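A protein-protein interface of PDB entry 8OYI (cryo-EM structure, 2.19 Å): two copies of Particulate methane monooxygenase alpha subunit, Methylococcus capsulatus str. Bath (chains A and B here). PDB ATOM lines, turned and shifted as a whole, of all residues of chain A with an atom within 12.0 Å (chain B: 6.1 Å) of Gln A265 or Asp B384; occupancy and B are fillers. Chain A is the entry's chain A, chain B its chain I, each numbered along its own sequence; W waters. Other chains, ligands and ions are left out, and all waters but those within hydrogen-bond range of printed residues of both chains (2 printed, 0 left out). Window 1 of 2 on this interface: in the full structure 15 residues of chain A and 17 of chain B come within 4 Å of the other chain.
OD1 of Asp B384 is in salt-bridge range of NH2 of Arg A112 (2.5 Å).
The backbone carbonyl oxygen of Asp B382 sits at hydrogen-bond distance from the side-chain amide nitrogen of Gln A265, at 3.3 Å.
N of Ser B385 is in hydrogen-bond range of OE1 of Gln A265.
N of Ala A266 is in hydrogen-bond range of O of Pro B383, 3.0 Å away.
The side-chain hydroxyl (OG) of Ser A113 sits at hydrogen-bond distance from the side-chain hydroxyl (OG1) of Thr A268, at 2.9 Å.
The side-chain amide nitrogen of Gln A265 lies within hydrogen-bond range of the backbone carbonyl oxygen of Pro A263 (3.0 Å).
NH1 of Arg A112 is in hydrogen-bond range of O of Ala A266, at 3.4 Å.
O of Met A269 lies within hydrogen-bond range of N of Arg A115 (3.2 Å).
The backbone NH (N) of Phe B41 is in hydrogen-bond range of the side-chain carboxylate (OD2) of Asp B382 (3.1 Å).
The guanidinium group (NH1) of Arg A112 sits at hydrogen-bond distance from the backbone carbonyl oxygen (O) of Gly A267, at 3.1 Å.
Among the printed residues, merely in contact across the chains: Arg A112 with Arg B386 (3.6 Å), Ile A262 with Ile B380 (3.9 Å), Pro A263 with Ile B380 (3.7 Å), Pro A263 with Asp B382 (3.4 Å), Pro A263 with Pro B383 (3.96 Å), Leu A264 with Pro B383 (3.4 Å), Gln A265 with Pro B383 (3.2 Å), Gln A265 with Asp B384 (3.7 Å), Ala A266 with Asp B384 (3.8 Å), Thr A268 with Arg B386 (3.8 Å) and Met A269 with Arg B386 (3.4 Å).
Gln A265 touches just these residues of chain B: Asp B382 (3.3 Å), Pro B383 (3.2 Å), Asp B384 (3.7 Å) and Ser B385 (3.0 Å).
Printed residues of chain B within 4 Å of Ala A266: Pro B383 (3.0 Å) and Asp B384 (3.8 Å).
Printed residues of chain B within 4 Å of Met A269: Arg B386.
Arg B45 touches none of the printed residues of chain A.
No residue of chain A comes within 4 Å of Ile B379.
Of chain A, only Pro A263 (3.96 Å), Leu A264 (3.4 Å), Gln A265 (3.2 Å) and Ala A266 (3.0 Å) come within 4 Å of Pro B383.
Asp B384 touches just these residues of chain A: Arg A112, Gln A265 and Ala A266.
Of chain A, only Gln A265 (3.0 Å) comes within 4 Å of Ser B385.
The nearest residue of chain B that does not touch Gln A265 is Arg B386 (5.8 Å).
The nearest residue of chain A that does not touch Asp B384 is Gly A267 (4.8 Å).
Hydrophobic or aromatic side chains of chain A that line the printed part of chain B: Ile A262, Pro A263 and Met A269.
Of the 11 printed residues of chain B, 6 touch a printed residue of chain A.
Printed residues of chain B that touch a printed residue of chain A: Ile B380, Asp B382, Pro B383, Asp B384, Ser B385 and Arg B386.
Hydrophobic or aromatic side chains of chain B that line the printed part of chain A: Pro B383.
Among the printed residues, Asp or Glu carboxylates within 4 Å of a Lys or Arg side-chain nitrogen of the other chain: Arg A112 with Asp B384 (2.5 Å).
No position is printed for both chains.
Of the 15 pairs that touch across the chains among the printed residues, none has its exchanged pair printed and touching as well.
Water W1 lies within hydrogen-bond range of N of Arg A270 (2.5 Å) and NH1 of Arg B386 (3.1 Å).
Water W2 lies within hydrogen-bond range of O of Thr A261 and O of Ile B380.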
ATOM      1  N   PHE A  88     -35.591  -5.207  35.455  1.00  0.00           N
ATOM      2  CA  PHE A  88     -36.117  -4.729  34.188  1.00  0.00           C
ATOM      3  C   PHE A  88     -37.627  -4.894  34.166  1.00  0.00           C
ATOM      4  O   PHE A  88     -38.142  -5.975  34.466  1.00  0.00           O
ATOM      5  CB  PHE A  88     -35.487  -5.479  33.012  1.00  0.00           C
ATOM      6  CG  PHE A  88     -35.949  -5.000  31.667  1.00  0.00           C
ATOM      7  CD1 PHE A  88     -35.592  -3.745  31.206  1.00  0.00           C
ATOM      8  CD2 PHE A  88     -36.743  -5.799  30.866  1.00  0.00           C
ATOM      9  CE1 PHE A  88     -36.016  -3.299  29.972  1.00  0.00           C
ATOM     10  CE2 PHE A  88     -37.170  -5.360  29.630  1.00  0.00           C
ATOM     11  CZ  PHE A  88     -36.806  -4.107  29.183  1.00  0.00           C
ATOM     12  N   ARG A 100     -43.463  -2.815  22.662  1.00  0.00           N
ATOM     13  CA  ARG A 100     -43.403  -1.931  23.821  1.00  0.00           C
ATOM     14  C   ARG A 100     -42.999  -0.542  23.346  1.00  0.00           C
ATOM     15  O   ARG A 100     -41.823  -0.270  23.096  1.00  0.00           O
ATOM     16  CB  ARG A 100     -42.424  -2.472  24.856  1.00  0.00           C
ATOM     17  CG  ARG A 100     -42.423  -1.704  26.165  1.00  0.00           C
ATOM     18  CD  ARG A 100     -41.305  -2.169  27.083  1.00  0.00           C
ATOM     19  NE  ARG A 100     -40.301  -2.951  26.375  1.00  0.00           N
ATOM     20  CZ  ARG A 100     -39.799  -4.097  26.810  1.00  0.00           C
ATOM     21  NH1 ARG A 100     -40.184  -4.627  27.961  1.00  0.00           N
ATOM     22  NH2 ARG A 100     -38.893  -4.731  26.074  1.00  0.00           N
ATOM     23  N   GLN A 108     -40.863   8.302  34.759  1.00  0.00           N
ATOM     24  CA  GLN A 108     -39.758   8.435  33.821  1.00  0.00           C
ATOM     25  C   GLN A 108     -39.560   7.152  33.024  1.00  0.00           C
ATOM     26  O   GLN A 108     -39.765   6.050  33.540  1.00  0.00           O
ATOM     27  CB  GLN A 108     -38.478   8.817  34.563  1.00  0.00           C
ATOM     28  CG  GLN A 108     -38.004   7.778  35.551  1.00  0.00           C
ATOM     29  CD  GLN A 108     -36.503   7.629  35.555  1.00  0.00           C
ATOM     30  OE1 GLN A 108     -35.935   6.990  34.674  1.00  0.00           O
ATOM     31  NE2 GLN A 108     -35.849   8.219  36.548  1.00  0.00           N
ATOM     32  N   LEU A 109     -39.163   7.310  31.763  1.00  0.00           N
ATOM     33  CA  LEU A 109     -39.023   6.174  30.862  1.00  0.00           C
ATOM     34  C   LEU A 109     -37.879   5.269  31.298  1.00  0.00           C
ATOM     35  O   LEU A 109     -36.825   5.737  31.733  1.00  0.00           O
ATOM     36  CB  LEU A 109     -38.792   6.673  29.433  1.00  0.00           C
ATOM     37  CG  LEU A 109     -38.872   5.638  28.312  1.00  0.00           C
ATOM     38  CD1 LEU A 109     -40.254   5.645  27.683  1.00  0.00           C
ATOM     39  CD2 LEU A 109     -37.804   5.902  27.270  1.00  0.00           C
ATOM     40  N   VAL A 110     -38.089   3.963  31.173  1.00  0.00           N
ATOM     41  CA  VAL A 110     -37.114   2.984  31.644  1.00  0.00           C
ATOM     42  C   VAL A 110     -36.803   1.973  30.544  1.00  0.00           C
ATOM     43  O   VAL A 110     -37.169   0.796  30.659  1.00  0.00           O
ATOM     44  CB  VAL A 110     -37.609   2.289  32.923  1.00  0.00           C
ATOM     45  CG1 VAL A 110     -37.472   3.227  34.104  1.00  0.00           C
ATOM     46  CG2 VAL A 110     -39.062   1.859  32.777  1.00  0.00           C
ATOM     47  N   PRO A 111     -36.116   2.372  29.468  1.00  0.00           N
ATOM     48  CA  PRO A 111     -35.753   1.397  28.432  1.00  0.00           C
ATOM     49  C   PRO A 111     -34.628   0.465  28.843  1.00  0.00           C
ATOM     50  O   PRO A 111     -34.369  -0.513  28.130  1.00  0.00           O
ATOM     51  CB  PRO A 111     -35.332   2.280  27.254  1.00  0.00           C
ATOM     52  CG  PRO A 111     -34.790   3.502  27.902  1.00  0.00           C
ATOM     53  CD  PRO A 111     -35.587   3.714  29.167  1.00  0.00           C
ATOM     54  N   ARG A 112     -33.956   0.734  29.954  1.00  0.00           N
ATOM     55  CA  ARG A 112     -32.860  -0.080  30.450  1.00  0.00           C
ATOM     56  C   ARG A 112     -33.245  -0.694  31.791  1.00  0.00           C
ATOM     57  O   ARG A 112     -34.331  -0.456  32.326  1.00  0.00           O
ATOM     58  CB  ARG A 112     -31.586   0.757  30.572  1.00  0.00           C
ATOM     59  CG  ARG A 112     -31.370   1.729  29.424  1.00  0.00           C
ATOM     60  CD  ARG A 112     -29.899   2.025  29.231  1.00  0.00           C
ATOM     61  NE  ARG A 112     -29.654   3.411  28.849  1.00  0.00           N
ATOM     62  CZ  ARG A 112     -28.892   4.248  29.535  1.00  0.00           C
ATOM     63  NH1 ARG A 112     -28.300   3.883  30.658  1.00  0.00           N
ATOM     64  NH2 ARG A 112     -28.714   5.485  29.079  1.00  0.00           N
ATOM     65  N   SER A 113     -32.339  -1.499  32.333  1.00  0.00           N
ATOM     66  CA  SER A 113     -32.545  -2.065  33.656  1.00  0.00           C
ATOM     67  C   SER A 113     -32.518  -0.964  34.709  1.00  0.00           C
ATOM     68  O   SER A 113     -31.889   0.081  34.529  1.00  0.00           O
ATOM     69  CB  SER A 113     -31.482  -3.117  33.959  1.00  0.00           C
ATOM     70  OG  SER A 113     -30.183  -2.619  33.696  1.00  0.00           O
ATOM     71  N   VAL A 114     -33.225  -1.201  35.811  1.00  0.00           N
ATOM     72  CA  VAL A 114     -33.359  -0.205  36.863  1.00  0.00           C
ATOM     73  C   VAL A 114     -33.056  -0.848  38.206  1.00  0.00           C
ATOM     74  O   VAL A 114     -33.066  -2.071  38.359  1.00  0.00           O
ATOM     75  CB  VAL A 114     -34.757   0.441  36.881  1.00  0.00           C
ATOM     76  CG1 VAL A 114     -35.077   1.042  35.530  1.00  0.00           C
ATOM     77  CG2 VAL A 114     -35.810  -0.575  37.282  1.00  0.00           C
ATOM     78  N   ARG A 115     -32.786   0.001  39.189  1.00  0.00           N
ATOM     79  CA  ARG A 115     -32.533  -0.432  40.554  1.00  0.00           C
ATOM     80  C   ARG A 115     -33.774  -0.177  41.396  1.00  0.00           C
ATOM     81  O   ARG A 115     -34.293   0.942  41.422  1.00  0.00           O
ATOM     82  CB  ARG A 115     -31.331   0.298  41.148  1.00  0.00           C
ATOM     83  CG  ARG A 115     -31.212   0.157  42.654  1.00  0.00           C
ATOM     84  CD  ARG A 115     -29.993   0.891  43.177  1.00  0.00           C
ATOM     85  NE  ARG A 115     -28.814   0.033  43.189  1.00  0.00           N
ATOM     86  CZ  ARG A 115     -28.343  -0.579  44.264  1.00  0.00           C
ATOM     87  NH1 ARG A 115     -28.926  -0.446  45.447  1.00  0.00           N
ATOM     88  NH2 ARG A 115     -27.261  -1.343  44.156  1.00  0.00           N
ATOM     89  N   LEU A 173     -32.211  11.391  14.812  1.00  0.00           N
ATOM     90  CA  LEU A 173     -31.635  12.718  14.977  1.00  0.00           C
ATOM     91  C   LEU A 173     -30.963  13.221  13.709  1.00  0.00           C
ATOM     92  O   LEU A 173     -30.582  14.397  13.653  1.00  0.00           O
ATOM     93  CB  LEU A 173     -30.638  12.722  16.135  1.00  0.00           C
ATOM     94  CG  LEU A 173     -31.266  12.633  17.525  1.00  0.00           C
ATOM     95  CD1 LEU A 173     -30.228  12.254  18.560  1.00  0.00           C
ATOM     96  CD2 LEU A 173     -31.932  13.949  17.892  1.00  0.00           C
ATOM     97  N   ILE A 260     -22.935   9.684  11.166  1.00  0.00           N
ATOM     98  CA  ILE A 260     -23.231   9.890  12.574  1.00  0.00           C
ATOM     99  C   ILE A 260     -23.782   8.580  13.127  1.00  0.00           C
ATOM    100  O   ILE A 260     -24.887   8.158  12.768  1.00  0.00           O
ATOM    101  CB  ILE A 260     -24.224  11.037  12.785  1.00  0.00           C
ATOM    102  CG1 ILE A 260     -23.584  12.374  12.396  1.00  0.00           C
ATOM    103  CG2 ILE A 260     -24.701  11.068  14.216  1.00  0.00           C
ATOM    104  CD1 ILE A 260     -24.370  13.145  11.367  1.00  0.00           C
ATOM    105  N   THR A 261     -23.011   7.936  13.996  1.00  0.00           N
ATOM    106  CA  THR A 261     -23.435   6.719  14.668  1.00  0.00           C
ATOM    107  C   THR A 261     -23.077   6.808  16.145  1.00  0.00           C
ATOM    108  O   THR A 261     -22.128   7.495  16.530  1.00  0.00           O
ATOM    109  CB  THR A 261     -22.794   5.458  14.059  1.00  0.00           C
ATOM    110  OG1 THR A 261     -21.368   5.543  14.162  1.00  0.00           O
ATOM    111  CG2 THR A 261     -23.193   5.289  12.603  1.00  0.00           C
ATOM    112  N   ILE A 262     -23.847   6.105  16.966  1.00  0.00           N
ATOM    113  CA  ILE A 262     -23.598   6.047  18.403  1.00  0.00           C
ATOM    114  C   ILE A 262     -23.556   4.583  18.821  1.00  0.00           C
ATOM    115  O   ILE A 262     -24.190   3.739  18.174  1.00  0.00           O
ATOM    116  CB  ILE A 262     -24.667   6.821  19.190  1.00  0.00           C
ATOM    117  CG1 ILE A 262     -26.064   6.285  18.871  1.00  0.00           C
ATOM    118  CG2 ILE A 262     -24.580   8.312  18.897  1.00  0.00           C
ATOM    119  CD1 ILE A 262     -27.056   6.472  19.993  1.00  0.00           C
ATOM    120  N   PRO A 263     -22.829   4.234  19.877  1.00  0.00           N
ATOM    121  CA  PRO A 263     -22.845   2.850  20.356  1.00  0.00           C
ATOM    122  C   PRO A 263     -24.184   2.508  20.991  1.00  0.00           C
ATOM    123  O   PRO A 263     -25.033   3.367  21.235  1.00  0.00           O
ATOM    124  CB  PRO A 263     -21.714   2.813  21.388  1.00  0.00           C
ATOM    125  CG  PRO A 263     -21.602   4.218  21.859  1.00  0.00           C
ATOM    126  CD  PRO A 263     -21.930   5.083  20.677  1.00  0.00           C
ATOM    127  N   LEU A 264     -24.367   1.216  21.247  1.00  0.00           N
ATOM    128  CA  LEU A 264     -25.563   0.753  21.936  1.00  0.00           C
ATOM    129  C   LEU A 264     -25.648   1.396  23.315  1.00  0.00           C
ATOM    130  O   LEU A 264     -24.663   1.435  24.056  1.00  0.00           O
ATOM    131  CB  LEU A 264     -25.546  -0.767  22.056  1.00  0.00           C
ATOM    132  CG  LEU A 264     -25.619  -1.528  20.733  1.00  0.00           C
ATOM    133  CD1 LEU A 264     -25.372  -3.007  20.950  1.00  0.00           C
ATOM    134  CD2 LEU A 264     -26.962  -1.299  20.070  1.00  0.00           C
ATOM    135  N   GLN A 265     -26.829   1.902  23.655  1.00  0.00           N
ATOM    136  CA  GLN A 265     -27.040   2.586  24.922  1.00  0.00           C
ATOM    137  C   GLN A 265     -27.484   1.571  25.970  1.00  0.00           C
ATOM    138  O   GLN A 265     -28.565   0.987  25.857  1.00  0.00           O
ATOM    139  CB  GLN A 265     -28.076   3.698  24.768  1.00  0.00           C
ATOM    140  CG  GLN A 265     -27.674   4.782  23.781  1.00  0.00           C
ATOM    141  CD  GLN A 265     -26.436   5.542  24.214  1.00  0.00           C
ATOM    142  OE1 GLN A 265     -26.509   6.453  25.034  1.00  0.00           O
ATOM    143  NE2 GLN A 265     -25.290   5.171  23.658  1.00  0.00           N
ATOM    144  N   ALA A 266     -26.648   1.366  26.984  1.00  0.00           N
ATOM    145  CA  ALA A 266     -26.914   0.367  28.006  1.00  0.00           C
ATOM    146  C   ALA A 266     -26.474   0.909  29.358  1.00  0.00           C
ATOM    147  O   ALA A 266     -25.790   1.931  29.452  1.00  0.00           O
ATOM    148  CB  ALA A 266     -26.203  -0.952  27.690  1.00  0.00           C
ATOM    149  N   GLY A 267     -26.891   0.212  30.410  1.00  0.00           N
ATOM    150  CA  GLY A 267     -26.516   0.583  31.761  1.00  0.00           C
ATOM    151  C   GLY A 267     -27.700   0.692  32.698  1.00  0.00           C
ATOM    152  O   GLY A 267     -28.696   1.344  32.371  1.00  0.00           O
ATOM    153  N   THR A 268     -27.602   0.055  33.864  1.00  0.00           N
ATOM    154  CA  THR A 268     -28.673   0.126  34.848  1.00  0.00           C
ATOM    155  C   THR A 268     -28.896   1.568  35.285  1.00  0.00           C
ATOM    156  O   THR A 268     -27.946   2.330  35.489  1.00  0.00           O
ATOM    157  CB  THR A 268     -28.341  -0.750  36.059  1.00  0.00           C
ATOM    158  OG1 THR A 268     -28.141  -2.101  35.629  1.00  0.00           O
ATOM    159  CG2 THR A 268     -29.471  -0.715  37.079  1.00  0.00           C
ATOM    160  N   MET A 269     -30.163   1.945  35.420  1.00  0.00           N
ATOM    161  CA  MET A 269     -30.548   3.307  35.754  1.00  0.00           C
ATOM    162  C   MET A 269     -30.939   3.366  37.226  1.00  0.00           C
ATOM    163  O   MET A 269     -31.841   2.646  37.664  1.00  0.00           O
ATOM    164  CB  MET A 269     -31.699   3.770  34.866  1.00  0.00           C
ATOM    165  CG  MET A 269     -31.270   4.092  33.443  1.00  0.00           C
ATOM    166  SD  MET A 269     -32.662   4.327  32.327  1.00  0.00           S
ATOM    167  CE  MET A 269     -33.591   5.559  33.223  1.00  0.00           C
ATOM    168  N   ARG A 270     -30.261   4.223  37.981  1.00  0.00           N
ATOM    169  CA  ARG A 270     -30.515   4.391  39.401  1.00  0.00           C
ATOM    170  C   ARG A 270     -31.516   5.519  39.623  1.00  0.00           C
ATOM    171  O   ARG A 270     -31.977   6.178  38.686  1.00  0.00           O
ATOM    172  CB  ARG A 270     -29.211   4.668  40.149  1.00  0.00           C
ATOM    173  CG  ARG A 270     -28.672   3.492  40.934  1.00  0.00           C
ATOM    174  CD  ARG A 270     -27.194   3.677  41.229  1.00  0.00           C
ATOM    175  NE  ARG A 270     -26.709   2.763  42.255  1.00  0.00           N
ATOM    176  CZ  ARG A 270     -26.945   2.894  43.553  1.00  0.00           C
ATOM    177  NH1 ARG A 270     -27.655   3.906  44.027  1.00  0.00           N
ATOM    178  NH2 ARG A 270     -26.455   1.993  44.396  1.00  0.00           N
ATOM    179  N   GLY A 271     -31.849   5.746  40.888  1.00  0.00           N
ATOM    180  CA  GLY A 271     -32.726   6.836  41.259  1.00  0.00           C
ATOM    181  C   GLY A 271     -34.144   6.711  40.747  1.00  0.00           C
ATOM    182  O   GLY A 271     -34.725   7.692  40.274  1.00  0.00           O
ATOM    183  N   MET A 272     -34.714   5.509  40.821  1.00  0.00           N
ATOM    184  CA  MET A 272     -36.138   5.326  40.564  1.00  0.00           C
ATOM    185  C   MET A 272     -36.912   5.964  41.707  1.00  0.00           C
ATOM    186  O   MET A 272     -36.609   5.726  42.879  1.00  0.00           O
ATOM    187  CB  MET A 272     -36.481   3.846  40.424  1.00  0.00           C
ATOM    188  CG  MET A 272     -35.777   3.124  39.283  1.00  0.00           C
ATOM    189  SD  MET A 272     -36.258   3.704  37.642  1.00  0.00           S
ATOM    190  CE  MET A 272     -34.962   4.887  37.277  1.00  0.00           C
ATOM    191  N   PHE B  41     -19.393  10.667  30.448  1.00  0.00           N
ATOM    192  CA  PHE B  41     -20.531  10.462  31.340  1.00  0.00           C
ATOM    193  C   PHE B  41     -20.085   9.875  32.670  1.00  0.00           C
ATOM    194  O   PHE B  41     -20.698  10.144  33.711  1.00  0.00           O
ATOM    195  CB  PHE B  41     -21.583   9.581  30.664  1.00  0.00           C
ATOM    196  CG  PHE B  41     -21.344   8.102  30.808  1.00  0.00           C
ATOM    197  CD1 PHE B  41     -20.525   7.431  29.918  1.00  0.00           C
ATOM    198  CD2 PHE B  41     -21.976   7.373  31.803  1.00  0.00           C
ATOM    199  CE1 PHE B  41     -20.317   6.068  30.032  1.00  0.00           C
ATOM    200  CE2 PHE B  41     -21.772   6.012  31.926  1.00  0.00           C
ATOM    201  CZ  PHE B  41     -20.945   5.358  31.034  1.00  0.00           C
ATOM    202  N   ARG B  45     -20.902  11.635  36.196  1.00  0.00           N
ATOM    203  CA  ARG B  45     -21.671  11.005  37.259  1.00  0.00           C
ATOM    204  C   ARG B  45     -20.821   9.956  37.966  1.00  0.00           C
ATOM    205  O   ARG B  45     -21.034   8.754  37.818  1.00  0.00           O
ATOM    206  CB  ARG B  45     -22.928  10.368  36.652  1.00  0.00           C
ATOM    207  CG  ARG B  45     -23.444  11.058  35.401  1.00  0.00           C
ATOM    208  CD  ARG B  45     -24.132  10.082  34.457  1.00  0.00           C
ATOM    209  NE  ARG B  45     -25.178   9.305  35.110  1.00  0.00           N
ATOM    210  CZ  ARG B  45     -26.415   9.734  35.322  1.00  0.00           C
ATOM    211  NH1 ARG B  45     -26.800  10.941  34.947  1.00  0.00           N
ATOM    212  NH2 ARG B  45     -27.285   8.930  35.923  1.00  0.00           N
ATOM    213  N   PRO B  78     -22.914   4.860  38.336  1.00  0.00           N
ATOM    214  CA  PRO B  78     -23.015   3.917  37.214  1.00  0.00           C
ATOM    215  C   PRO B  78     -22.850   2.477  37.680  1.00  0.00           C
ATOM    216  O   PRO B  78     -22.031   2.179  38.550  1.00  0.00           O
ATOM    217  CB  PRO B  78     -21.876   4.350  36.284  1.00  0.00           C
ATOM    218  CG  PRO B  78     -20.930   5.100  37.155  1.00  0.00           C
ATOM    219  CD  PRO B  78     -21.755   5.757  38.214  1.00  0.00           C
ATOM    220  N   ILE B 379     -18.943  12.594  24.800  1.00  0.00           N
ATOM    221  CA  ILE B 379     -20.037  11.759  25.381  1.00  0.00           C
ATOM    222  C   ILE B 379     -20.811  11.137  24.210  1.00  0.00           C
ATOM    223  O   ILE B 379     -21.578  10.182  24.442  1.00  0.00           O
ATOM    224  CB  ILE B 379     -20.909  12.593  26.346  1.00  0.00           C
ATOM    225  CG1 ILE B 379     -21.902  11.735  27.138  1.00  0.00           C
ATOM    226  CG2 ILE B 379     -21.598  13.734  25.616  1.00  0.00           C
ATOM    227  CD1 ILE B 379     -22.613  12.471  28.243  1.00  0.00           C
ATOM    228  N   ILE B 380     -20.584  11.618  22.981  1.00  0.00           N
ATOM    229  CA  ILE B 380     -21.230  10.983  21.837  1.00  0.00           C
ATOM    230  C   ILE B 380     -20.664   9.587  21.603  1.00  0.00           C
ATOM    231  O   ILE B 380     -21.341   8.722  21.035  1.00  0.00           O
ATOM    232  CB  ILE B 380     -21.091  11.876  20.588  1.00  0.00           C
ATOM    233  CG1 ILE B 380     -22.079  11.443  19.503  1.00  0.00           C
ATOM    234  CG2 ILE B 380     -19.658  11.868  20.067  1.00  0.00           C
ATOM    235  CD1 ILE B 380     -21.815  12.070  18.159  1.00  0.00           C
ATOM    236  N   ASP B 382     -19.854   7.645  24.140  1.00  0.00           N
ATOM    237  CA  ASP B 382     -20.170   6.873  25.329  1.00  0.00           C
ATOM    238  C   ASP B 382     -21.414   6.012  25.118  1.00  0.00           C
ATOM    239  O   ASP B 382     -22.325   6.392  24.379  1.00  0.00           O
ATOM    240  CB  ASP B 382     -20.384   7.800  26.516  1.00  0.00           C
ATOM    241  CG  ASP B 382     -19.088   8.400  27.029  1.00  0.00           C
ATOM    242  OD1 ASP B 382     -18.024   7.776  26.825  1.00  0.00           O
ATOM    243  OD2 ASP B 382     -19.133   9.487  27.638  1.00  0.00           O
ATOM    244  N   PRO B 383     -21.475   4.848  25.767  1.00  0.00           N
ATOM    245  CA  PRO B 383     -22.677   4.013  25.706  1.00  0.00           C
ATOM    246  C   PRO B 383     -23.783   4.427  26.665  1.00  0.00           C
ATOM    247  O   PRO B 383     -24.762   3.687  26.803  1.00  0.00           O
ATOM    248  CB  PRO B 383     -22.134   2.625  26.076  1.00  0.00           C
ATOM    249  CG  PRO B 383     -21.011   2.917  26.998  1.00  0.00           C
ATOM    250  CD  PRO B 383     -20.382   4.191  26.505  1.00  0.00           C
ATOM    251  N   ASP B 384     -23.652   5.568  27.338  1.00  0.00           N
ATOM    252  CA  ASP B 384     -24.690   6.054  28.246  1.00  0.00           C
ATOM    253  C   ASP B 384     -24.651   7.579  28.191  1.00  0.00           C
ATOM    254  O   ASP B 384     -23.867   8.207  28.906  1.00  0.00           O
ATOM    255  CB  ASP B 384     -24.473   5.538  29.663  1.00  0.00           C
ATOM    256  CG  ASP B 384     -25.676   5.761  30.557  1.00  0.00           C
ATOM    257  OD1 ASP B 384     -26.648   6.406  30.112  1.00  0.00           O
ATOM    258  OD2 ASP B 384     -25.649   5.290  31.713  1.00  0.00           O
ATOM    259  N   SER B 385     -25.505   8.163  27.351  1.00  0.00           N
ATOM    260  CA  SER B 385     -25.511   9.611  27.137  1.00  0.00           C
ATOM    261  C   SER B 385     -26.407  10.285  28.177  1.00  0.00           C
ATOM    262  O   SER B 385     -27.490  10.798  27.888  1.00  0.00           O
ATOM    263  CB  SER B 385     -25.954   9.938  25.721  1.00  0.00           C
ATOM    264  OG  SER B 385     -25.476  11.212  25.322  1.00  0.00           O
ATOM    265  N   ARG B 386     -25.924  10.272  29.414  1.00  0.00           N
ATOM    266  CA  ARG B 386     -26.568  10.970  30.512  1.00  0.00           C
ATOM    267  C   ARG B 386     -25.524  11.795  31.245  1.00  0.00           C
ATOM    268  O   ARG B 386     -24.387  11.358  31.440  1.00  0.00           O
ATOM    269  CB  ARG B 386     -27.252   9.998  31.482  1.00  0.00           C
ATOM    270  CG  ARG B 386     -28.510   9.355  30.925  1.00  0.00           C
ATOM    271  CD  ARG B 386     -29.176   8.458  31.951  1.00  0.00           C
ATOM    272  NE  ARG B 386     -28.306   7.369  32.372  1.00  0.00           N
ATOM    273  CZ  ARG B 386     -28.497   6.639  33.464  1.00  0.00           C
ATOM    274  NH1 ARG B 386     -29.524   6.851  34.265  1.00  0.00           N
ATOM    275  NH2 ARG B 386     -27.632   5.669  33.754  1.00  0.00           N
ATOM    276  N   PHE B 387     -25.913  13.003  31.634  1.00  0.00           N
ATOM    277  CA  PHE B 387     -25.023  13.906  32.340  1.00  0.00           C
ATOM    278  C   PHE B 387     -25.531  14.130  33.756  1.00  0.00           C
ATOM    279  O   PHE B 387     -26.705  13.912  34.061  1.00  0.00           O
ATOM    280  CB  PHE B 387     -24.892  15.253  31.607  1.00  0.00           C
ATOM    281  CG  PHE B 387     -25.915  16.273  32.023  1.00  0.00           C
ATOM    282  CD1 PHE B 387     -27.169  16.289  31.438  1.00  0.00           C
ATOM    283  CD2 PHE B 387     -25.622  17.226  32.987  1.00  0.00           C
ATOM    284  CE1 PHE B 387     -28.112  17.222  31.814  1.00  0.00           C
ATOM    285  CE2 PHE B 387     -26.564  18.161  33.370  1.00  0.00           C
ATOM    286  CZ  PHE B 387     -27.809  18.162  32.778  1.00  0.00           C
HETATM  287  O   HOH W   1     -28.630   5.883  37.023  1.00  0.00           O
HETATM  288  O   HOH W   2     -20.432   8.070  18.408  1.00  0.00           O
